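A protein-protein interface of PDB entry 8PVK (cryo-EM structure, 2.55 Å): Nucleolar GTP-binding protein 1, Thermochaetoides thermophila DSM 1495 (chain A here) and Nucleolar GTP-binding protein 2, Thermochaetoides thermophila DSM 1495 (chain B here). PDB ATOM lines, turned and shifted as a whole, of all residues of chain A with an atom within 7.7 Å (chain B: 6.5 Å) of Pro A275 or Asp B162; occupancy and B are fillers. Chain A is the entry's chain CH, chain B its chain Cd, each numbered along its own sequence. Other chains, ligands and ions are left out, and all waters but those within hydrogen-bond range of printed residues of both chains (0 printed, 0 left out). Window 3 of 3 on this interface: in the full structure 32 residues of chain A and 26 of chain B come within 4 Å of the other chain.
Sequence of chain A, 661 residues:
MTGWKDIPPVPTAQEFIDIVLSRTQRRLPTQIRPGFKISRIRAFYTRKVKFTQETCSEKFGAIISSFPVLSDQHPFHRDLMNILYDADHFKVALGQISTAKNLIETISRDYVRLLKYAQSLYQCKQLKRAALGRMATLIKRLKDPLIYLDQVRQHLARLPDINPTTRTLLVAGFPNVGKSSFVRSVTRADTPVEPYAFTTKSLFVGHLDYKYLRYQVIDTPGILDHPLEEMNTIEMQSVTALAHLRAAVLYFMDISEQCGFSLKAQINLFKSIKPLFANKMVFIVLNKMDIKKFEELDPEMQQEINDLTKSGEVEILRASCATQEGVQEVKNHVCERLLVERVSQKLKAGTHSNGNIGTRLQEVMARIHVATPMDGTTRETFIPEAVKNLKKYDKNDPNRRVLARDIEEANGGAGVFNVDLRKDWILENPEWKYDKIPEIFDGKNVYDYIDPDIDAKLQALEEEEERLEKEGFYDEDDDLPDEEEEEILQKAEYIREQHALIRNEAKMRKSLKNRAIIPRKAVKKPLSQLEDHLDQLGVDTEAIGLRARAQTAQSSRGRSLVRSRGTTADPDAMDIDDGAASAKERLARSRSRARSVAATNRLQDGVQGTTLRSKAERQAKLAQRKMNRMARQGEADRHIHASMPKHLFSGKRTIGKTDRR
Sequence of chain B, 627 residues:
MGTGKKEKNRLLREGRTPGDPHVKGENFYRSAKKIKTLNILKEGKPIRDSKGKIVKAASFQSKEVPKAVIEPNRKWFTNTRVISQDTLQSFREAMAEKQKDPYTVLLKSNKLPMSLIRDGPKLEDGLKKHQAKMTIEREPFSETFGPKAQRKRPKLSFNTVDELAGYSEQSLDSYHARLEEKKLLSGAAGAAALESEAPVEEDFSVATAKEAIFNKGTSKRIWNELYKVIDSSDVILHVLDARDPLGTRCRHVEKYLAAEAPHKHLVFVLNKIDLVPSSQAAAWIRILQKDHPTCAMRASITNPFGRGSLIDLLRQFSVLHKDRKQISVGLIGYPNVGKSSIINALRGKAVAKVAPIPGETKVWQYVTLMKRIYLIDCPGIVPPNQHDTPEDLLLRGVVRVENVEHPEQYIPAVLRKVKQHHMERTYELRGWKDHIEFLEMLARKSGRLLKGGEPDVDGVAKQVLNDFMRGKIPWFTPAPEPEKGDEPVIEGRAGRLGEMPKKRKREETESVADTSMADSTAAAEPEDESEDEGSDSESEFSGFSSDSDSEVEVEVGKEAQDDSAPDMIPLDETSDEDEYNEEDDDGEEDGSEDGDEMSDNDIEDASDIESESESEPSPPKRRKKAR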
ATOM      1  N   LEU A 228     -27.120 -18.194  -0.273  1.00  0.00           N
ATOM      2  CA  LEU A 228     -27.784 -17.729  -1.485  1.00  0.00           C
ATOM      3  C   LEU A 228     -29.068 -18.489  -1.781  1.00  0.00           C
ATOM      4  O   LEU A 228     -29.965 -17.933  -2.424  1.00  0.00           O
ATOM      5  CB  LEU A 228     -26.829 -17.842  -2.676  1.00  0.00           C
ATOM      6  CG  LEU A 228     -26.007 -16.611  -3.067  1.00  0.00           C
ATOM      7  CD1 LEU A 228     -25.026 -16.218  -1.974  1.00  0.00           C
ATOM      8  CD2 LEU A 228     -25.268 -16.871  -4.365  1.00  0.00           C
ATOM      9  N   LEU A 242     -23.420  -6.777  -6.909  1.00  0.00           N
ATOM     10  CA  LEU A 242     -22.069  -7.050  -6.428  1.00  0.00           C
ATOM     11  C   LEU A 242     -21.333  -8.040  -7.321  1.00  0.00           C
ATOM     12  O   LEU A 242     -20.112  -7.946  -7.472  1.00  0.00           O
ATOM     13  CB  LEU A 242     -22.108  -7.581  -4.996  1.00  0.00           C
ATOM     14  CG  LEU A 242     -22.433  -6.605  -3.867  1.00  0.00           C
ATOM     15  CD1 LEU A 242     -22.656  -7.374  -2.583  1.00  0.00           C
ATOM     16  CD2 LEU A 242     -21.317  -5.597  -3.692  1.00  0.00           C
ATOM     17  N   LEU A 269     -20.638 -11.495   7.166  1.00  0.00           N
ATOM     18  CA  LEU A 269     -21.199 -11.211   5.847  1.00  0.00           C
ATOM     19  C   LEU A 269     -20.128 -10.694   4.894  1.00  0.00           C
ATOM     20  O   LEU A 269     -20.089 -11.087   3.719  1.00  0.00           O
ATOM     21  CB  LEU A 269     -22.341 -10.201   5.956  1.00  0.00           C
ATOM     22  CG  LEU A 269     -22.934  -9.775   4.606  1.00  0.00           C
ATOM     23  CD1 LEU A 269     -23.579 -10.963   3.907  1.00  0.00           C
ATOM     24  CD2 LEU A 269     -23.915  -8.624   4.739  1.00  0.00           C
ATOM     25  N   PHE A 270     -19.247  -9.816   5.390  1.00  0.00           N
ATOM     26  CA  PHE A 270     -18.149  -9.322   4.562  1.00  0.00           C
ATOM     27  C   PHE A 270     -17.225 -10.455   4.130  1.00  0.00           C
ATOM     28  O   PHE A 270     -16.822 -10.525   2.965  1.00  0.00           O
ATOM     29  CB  PHE A 270     -17.361  -8.249   5.313  1.00  0.00           C
ATOM     30  CG  PHE A 270     -16.174  -7.733   4.554  1.00  0.00           C
ATOM     31  CD1 PHE A 270     -16.341  -6.848   3.504  1.00  0.00           C
ATOM     32  CD2 PHE A 270     -14.889  -8.132   4.891  1.00  0.00           C
ATOM     33  CE1 PHE A 270     -15.254  -6.373   2.801  1.00  0.00           C
ATOM     34  CE2 PHE A 270     -13.796  -7.659   4.190  1.00  0.00           C
ATOM     35  CZ  PHE A 270     -13.980  -6.777   3.144  1.00  0.00           C
ATOM     36  N   LYS A 271     -16.896 -11.364   5.052  1.00  0.00           N
ATOM     37  CA  LYS A 271     -16.042 -12.496   4.707  1.00  0.00           C
ATOM     38  C   LYS A 271     -16.731 -13.454   3.740  1.00  0.00           C
ATOM     39  O   LYS A 271     -16.063 -14.074   2.906  1.00  0.00           O
ATOM     40  CB  LYS A 271     -15.615 -13.240   5.971  1.00  0.00           C
ATOM     41  CG  LYS A 271     -14.662 -12.462   6.861  1.00  0.00           C
ATOM     42  CD  LYS A 271     -14.384 -13.215   8.150  1.00  0.00           C
ATOM     43  CE  LYS A 271     -13.296 -12.537   8.963  1.00  0.00           C
ATOM     44  NZ  LYS A 271     -13.114 -13.181  10.292  1.00  0.00           N
ATOM     45  N   SER A 272     -18.056 -13.587   3.836  1.00  0.00           N
ATOM     46  CA  SER A 272     -18.772 -14.492   2.944  1.00  0.00           C
ATOM     47  C   SER A 272     -18.882 -13.922   1.535  1.00  0.00           C
ATOM     48  O   SER A 272     -18.835 -14.672   0.553  1.00  0.00           O
ATOM     49  CB  SER A 272     -20.159 -14.795   3.509  1.00  0.00           C
ATOM     50  OG  SER A 272     -20.972 -13.635   3.509  1.00  0.00           O
ATOM     51  N   ILE A 273     -19.034 -12.604   1.408  1.00  0.00           N
ATOM     52  CA  ILE A 273     -19.186 -11.994   0.089  1.00  0.00           C
ATOM     53  C   ILE A 273     -17.852 -11.456  -0.421  1.00  0.00           C
ATOM     54  O   ILE A 273     -17.792 -10.808  -1.473  1.00  0.00           O
ATOM     55  CB  ILE A 273     -20.272 -10.901   0.113  1.00  0.00           C
ATOM     56  CG1 ILE A 273     -19.767  -9.626   0.790  1.00  0.00           C
ATOM     57  CG2 ILE A 273     -21.537 -11.420   0.777  1.00  0.00           C
ATOM     58  CD1 ILE A 273     -20.759  -8.488   0.740  1.00  0.00           C
ATOM     59  N   LYS A 274     -16.780 -11.719   0.326  1.00  0.00           N
ATOM     60  CA  LYS A 274     -15.432 -11.437  -0.165  1.00  0.00           C
ATOM     61  C   LYS A 274     -15.062 -12.101  -1.497  1.00  0.00           C
ATOM     62  O   LYS A 274     -14.387 -11.433  -2.300  1.00  0.00           O
ATOM     63  CB  LYS A 274     -14.412 -11.796   0.929  1.00  0.00           C
ATOM     64  CG  LYS A 274     -12.982 -11.380   0.624  1.00  0.00           C
ATOM     65  CD  LYS A 274     -12.025 -11.854   1.704  1.00  0.00           C
ATOM     66  CE  LYS A 274     -12.147 -11.005   2.959  1.00  0.00           C
ATOM     67  NZ  LYS A 274     -11.123 -11.370   3.976  1.00  0.00           N
ATOM     68  N   PRO A 275     -15.410 -13.371  -1.796  1.00  0.00           N
ATOM     69  CA  PRO A 275     -15.054 -13.913  -3.124  1.00  0.00           C
ATOM     70  C   PRO A 275     -15.670 -13.178  -4.305  1.00  0.00           C
ATOM     71  O   PRO A 275     -15.120 -13.245  -5.412  1.00  0.00           O
ATOM     72  CB  PRO A 275     -15.552 -15.361  -3.054  1.00  0.00           C
ATOM     73  CG  PRO A 275     -15.463 -15.705  -1.641  1.00  0.00           C
ATOM     74  CD  PRO A 275     -15.862 -14.465  -0.907  1.00  0.00           C
ATOM     75  N   LEU A 276     -16.791 -12.480  -4.115  1.00  0.00           N
ATOM     76  CA  LEU A 276     -17.341 -11.659  -5.189  1.00  0.00           C
ATOM     77  C   LEU A 276     -16.523 -10.399  -5.433  1.00  0.00           C
ATOM     78  O   LEU A 276     -16.714  -9.740  -6.461  1.00  0.00           O
ATOM     79  CB  LEU A 276     -18.788 -11.275  -4.880  1.00  0.00           C
ATOM     80  CG  LEU A 276     -19.840 -12.356  -5.113  1.00  0.00           C
ATOM     81  CD1 LEU A 276     -21.229 -11.821  -4.811  1.00  0.00           C
ATOM     82  CD2 LEU A 276     -19.755 -12.874  -6.537  1.00  0.00           C
ATOM     83  N   PHE A 277     -15.624 -10.049  -4.518  1.00  0.00           N
ATOM     84  CA  PHE A 277     -14.850  -8.820  -4.602  1.00  0.00           C
ATOM     85  C   PHE A 277     -13.517  -9.006  -5.311  1.00  0.00           C
ATOM     86  O   PHE A 277     -12.687  -8.091  -5.281  1.00  0.00           O
ATOM     87  CB  PHE A 277     -14.609  -8.254  -3.201  1.00  0.00           C
ATOM     88  CG  PHE A 277     -15.861  -7.812  -2.502  1.00  0.00           C
ATOM     89  CD1 PHE A 277     -16.981  -7.432  -3.223  1.00  0.00           C
ATOM     90  CD2 PHE A 277     -15.914  -7.771  -1.118  1.00  0.00           C
ATOM     91  CE1 PHE A 277     -18.131  -7.030  -2.580  1.00  0.00           C
ATOM     92  CE2 PHE A 277     -17.061  -7.366  -0.469  1.00  0.00           C
ATOM     93  CZ  PHE A 277     -18.170  -6.993  -1.202  1.00  0.00           C
ATOM     94  N   ALA A 278     -13.282 -10.169  -5.912  1.00  0.00           N
ATOM     95  CA  ALA A 278     -12.062 -10.391  -6.675  1.00  0.00           C
ATOM     96  C   ALA A 278     -12.034  -9.485  -7.897  1.00  0.00           C
ATOM     97  O   ALA A 278     -13.074  -9.209  -8.504  1.00  0.00           O
ATOM     98  CB  ALA A 278     -11.955 -11.855  -7.099  1.00  0.00           C
ATOM     99  N   ASN A 279     -10.829  -9.013  -8.240  1.00  0.00           N
ATOM    100  CA  ASN A 279     -10.605  -8.015  -9.291  1.00  0.00           C
ATOM    101  C   ASN A 279     -11.416  -6.744  -9.050  1.00  0.00           C
ATOM    102  O   ASN A 279     -11.928  -6.136  -9.992  1.00  0.00           O
ATOM    103  CB  ASN A 279     -10.896  -8.587 -10.687  1.00  0.00           C
ATOM    104  CG  ASN A 279     -10.026  -7.971 -11.770  1.00  0.00           C
ATOM    105  OD1 ASN A 279      -9.204  -7.096 -11.500  1.00  0.00           O
ATOM    106  ND2 ASN A 279     -10.199  -8.434 -13.004  1.00  0.00           N
ATOM    107  N   LYS A 280     -11.552  -6.326  -7.790  1.00  0.00           N
ATOM    108  CA  LYS A 280     -12.296  -5.117  -7.464  1.00  0.00           C
ATOM    109  C   LYS A 280     -11.590  -4.326  -6.373  1.00  0.00           C
ATOM    110  O   LYS A 280     -10.426  -4.565  -6.043  1.00  0.00           O
ATOM    111  CB  LYS A 280     -13.740  -5.396  -7.025  1.00  0.00           C
ATOM    112  CG  LYS A 280     -14.675  -5.883  -8.109  1.00  0.00           C
ATOM    113  CD  LYS A 280     -16.084  -5.959  -7.556  1.00  0.00           C
ATOM    114  CE  LYS A 280     -17.030  -6.679  -8.487  1.00  0.00           C
ATOM    115  NZ  LYS A 280     -18.427  -6.494  -8.022  1.00  0.00           N
ATOM    116  N   THR B 160     -23.213 -21.405  -4.571  1.00  0.00           N
ATOM    117  CA  THR B 160     -22.326 -20.728  -3.638  1.00  0.00           C
ATOM    118  C   THR B 160     -21.768 -19.451  -4.257  1.00  0.00           C
ATOM    119  O   THR B 160     -21.956 -19.161  -5.442  1.00  0.00           O
ATOM    120  CB  THR B 160     -21.173 -21.642  -3.200  1.00  0.00           C
ATOM    121  OG1 THR B 160     -20.296 -21.876  -4.309  1.00  0.00           O
ATOM    122  CG2 THR B 160     -21.704 -22.971  -2.689  1.00  0.00           C
ATOM    123  N   VAL B 161     -21.066 -18.691  -3.414  1.00  0.00           N
ATOM    124  CA  VAL B 161     -20.475 -17.424  -3.832  1.00  0.00           C
ATOM    125  C   VAL B 161     -19.336 -17.658  -4.820  1.00  0.00           C
ATOM    126  O   VAL B 161     -19.161 -16.898  -5.781  1.00  0.00           O
ATOM    127  CB  VAL B 161     -20.015 -16.638  -2.588  1.00  0.00           C
ATOM    128  CG1 VAL B 161     -19.320 -15.346  -2.973  1.00  0.00           C
ATOM    129  CG2 VAL B 161     -21.202 -16.354  -1.681  1.00  0.00           C
ATOM    130  N   ASP B 162     -18.549 -18.717  -4.605  1.00  0.00           N
ATOM    131  CA  ASP B 162     -17.474 -19.055  -5.536  1.00  0.00           C
ATOM    132  C   ASP B 162     -18.029 -19.444  -6.902  1.00  0.00           C
ATOM    133  O   ASP B 162     -17.493 -19.032  -7.944  1.00  0.00           O
ATOM    134  CB  ASP B 162     -16.633 -20.193  -4.962  1.00  0.00           C
ATOM    135  CG  ASP B 162     -15.936 -19.810  -3.674  1.00  0.00           C
ATOM    136  OD1 ASP B 162     -15.600 -18.620  -3.510  1.00  0.00           O
ATOM    137  OD2 ASP B 162     -15.731 -20.698  -2.820  1.00  0.00           O
ATOM    138  N   GLU B 163     -19.106 -20.234  -6.912  1.00  0.00           N
ATOM    139  CA  GLU B 163     -19.768 -20.585  -8.163  1.00  0.00           C
ATOM    140  C   GLU B 163     -20.348 -19.352  -8.838  1.00  0.00           C
ATOM    141  O   GLU B 163     -20.318 -19.244 -10.065  1.00  0.00           O
ATOM    142  CB  GLU B 163     -20.866 -21.616  -7.914  1.00  0.00           C
ATOM    143  CG  GLU B 163     -20.368 -22.961  -7.426  1.00  0.00           C
ATOM    144  CD  GLU B 163     -21.505 -23.907  -7.106  1.00  0.00           C
ATOM    145  OE1 GLU B 163     -22.674 -23.494  -7.247  1.00  0.00           O
ATOM    146  OE2 GLU B 163     -21.233 -25.060  -6.712  1.00  0.00           O
ATOM    147  N   LEU B 164     -20.875 -18.411  -8.049  1.00  0.00           N
ATOM    148  CA  LEU B 164     -21.390 -17.167  -8.613  1.00  0.00           C
ATOM    149  C   LEU B 164     -20.278 -16.340  -9.250  1.00  0.00           C
ATOM    150  O   LEU B 164     -20.473 -15.750 -10.318  1.00  0.00           O
ATOM    151  CB  LEU B 164     -22.106 -16.361  -7.530  1.00  0.00           C
ATOM    152  CG  LEU B 164     -22.562 -14.936  -7.857  1.00  0.00           C
ATOM    153  CD1 LEU B 164     -23.421 -14.870  -9.112  1.00  0.00           C
ATOM    154  CD2 LEU B 164     -23.304 -14.358  -6.675  1.00  0.00           C
ATOM    155  N   ALA B 165     -19.109 -16.282  -8.608  1.00  0.00           N
ATOM    156  CA  ALA B 165     -17.986 -15.531  -9.165  1.00  0.00           C
ATOM    157  C   ALA B 165     -17.496 -16.152 -10.471  1.00  0.00           C
ATOM    158  O   ALA B 165     -17.268 -15.444 -11.465  1.00  0.00           O
ATOM    159  CB  ALA B 165     -16.850 -15.453  -8.145  1.00  0.00           C
ATOM    160  N   GLY B 166     -17.344 -17.481 -10.488  1.00  0.00           N
ATOM    161  CA  GLY B 166     -16.954 -18.155 -11.719  1.00  0.00           C
ATOM    162  C   GLY B 166     -17.994 -18.020 -12.817  1.00  0.00           C
ATOM    163  O   GLY B 166     -17.655 -17.835 -13.990  1.00  0.00           O
ATOM    164  N   TYR B 167     -19.275 -18.091 -12.444  1.00  0.00           N
ATOM    165  CA  TYR B 167     -20.365 -17.925 -13.395  1.00  0.00           C
ATOM    166  C   TYR B 167     -20.387 -16.519 -13.975  1.00  0.00           C
ATOM    167  O   TYR B 167     -20.638 -16.346 -15.170  1.00  0.00           O
ATOM    168  CB  TYR B 167     -21.693 -18.248 -12.710  1.00  0.00           C
ATOM    169  CG  TYR B 167     -22.902 -18.150 -13.609  1.00  0.00           C
ATOM    170  CD1 TYR B 167     -23.179 -19.139 -14.542  1.00  0.00           C
ATOM    171  CD2 TYR B 167     -23.775 -17.074 -13.515  1.00  0.00           C
ATOM    172  CE1 TYR B 167     -24.286 -19.056 -15.363  1.00  0.00           C
ATOM    173  CE2 TYR B 167     -24.885 -16.981 -14.331  1.00  0.00           C
ATOM    174  CZ  TYR B 167     -25.135 -17.975 -15.253  1.00  0.00           C
ATOM    175  OH  TYR B 167     -26.240 -17.888 -16.068  1.00  0.00           O
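Of the printed residues of chain A, Asp B162 touches Pro A275.
Of the printed residues of chain A, Ala B165 touches Pro A275 (3.9 Å).
Printed residues of chain B within 4 Å of Ser A272: Val B161 (3.6 Å).
Printed residues of chain B within 4 Å of Leu A276: Val B161 (3.7 Å) and Leu B164 (3.7 Å).
Leu A242 touches none of the printed residues of chain B.
The nearest printed residue of chain A that does not touch Leu B164 is Leu A242 (6.6 Å).
The backbone carbonyl oxygen (O) of Leu A269 sits at hydrogen-bond distance from the side-chain hydroxyl (OG) of Ser A272, at 2.7 Å.
Among the printed residues, merely in contact across the chains: Leu A228 with Val B161 (3.8 Å), Leu A228 with Leu B164 (3.9 Å), Ser A272 with Val B161 (3.6 Å), Pro A275 with Val B161 (3.8 Å), Pro A275 with Asp B162 (3.3 Å), Pro A275 with Ala B165 (3.9 Å), Leu A276 with Val B161 (3.7 Å) and Leu A276 with Leu B164 (3.7 Å).
Of the 8 printed residues of chain B, 4 touch a printed residue of chain A.
Hydrophobic or aromatic side chains of chain B that line the printed part of chain A: Val B161, Leu B164 and Ala B165.
Of the 14 printed residues of chain A, 4 touch a printed residue of chain B.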
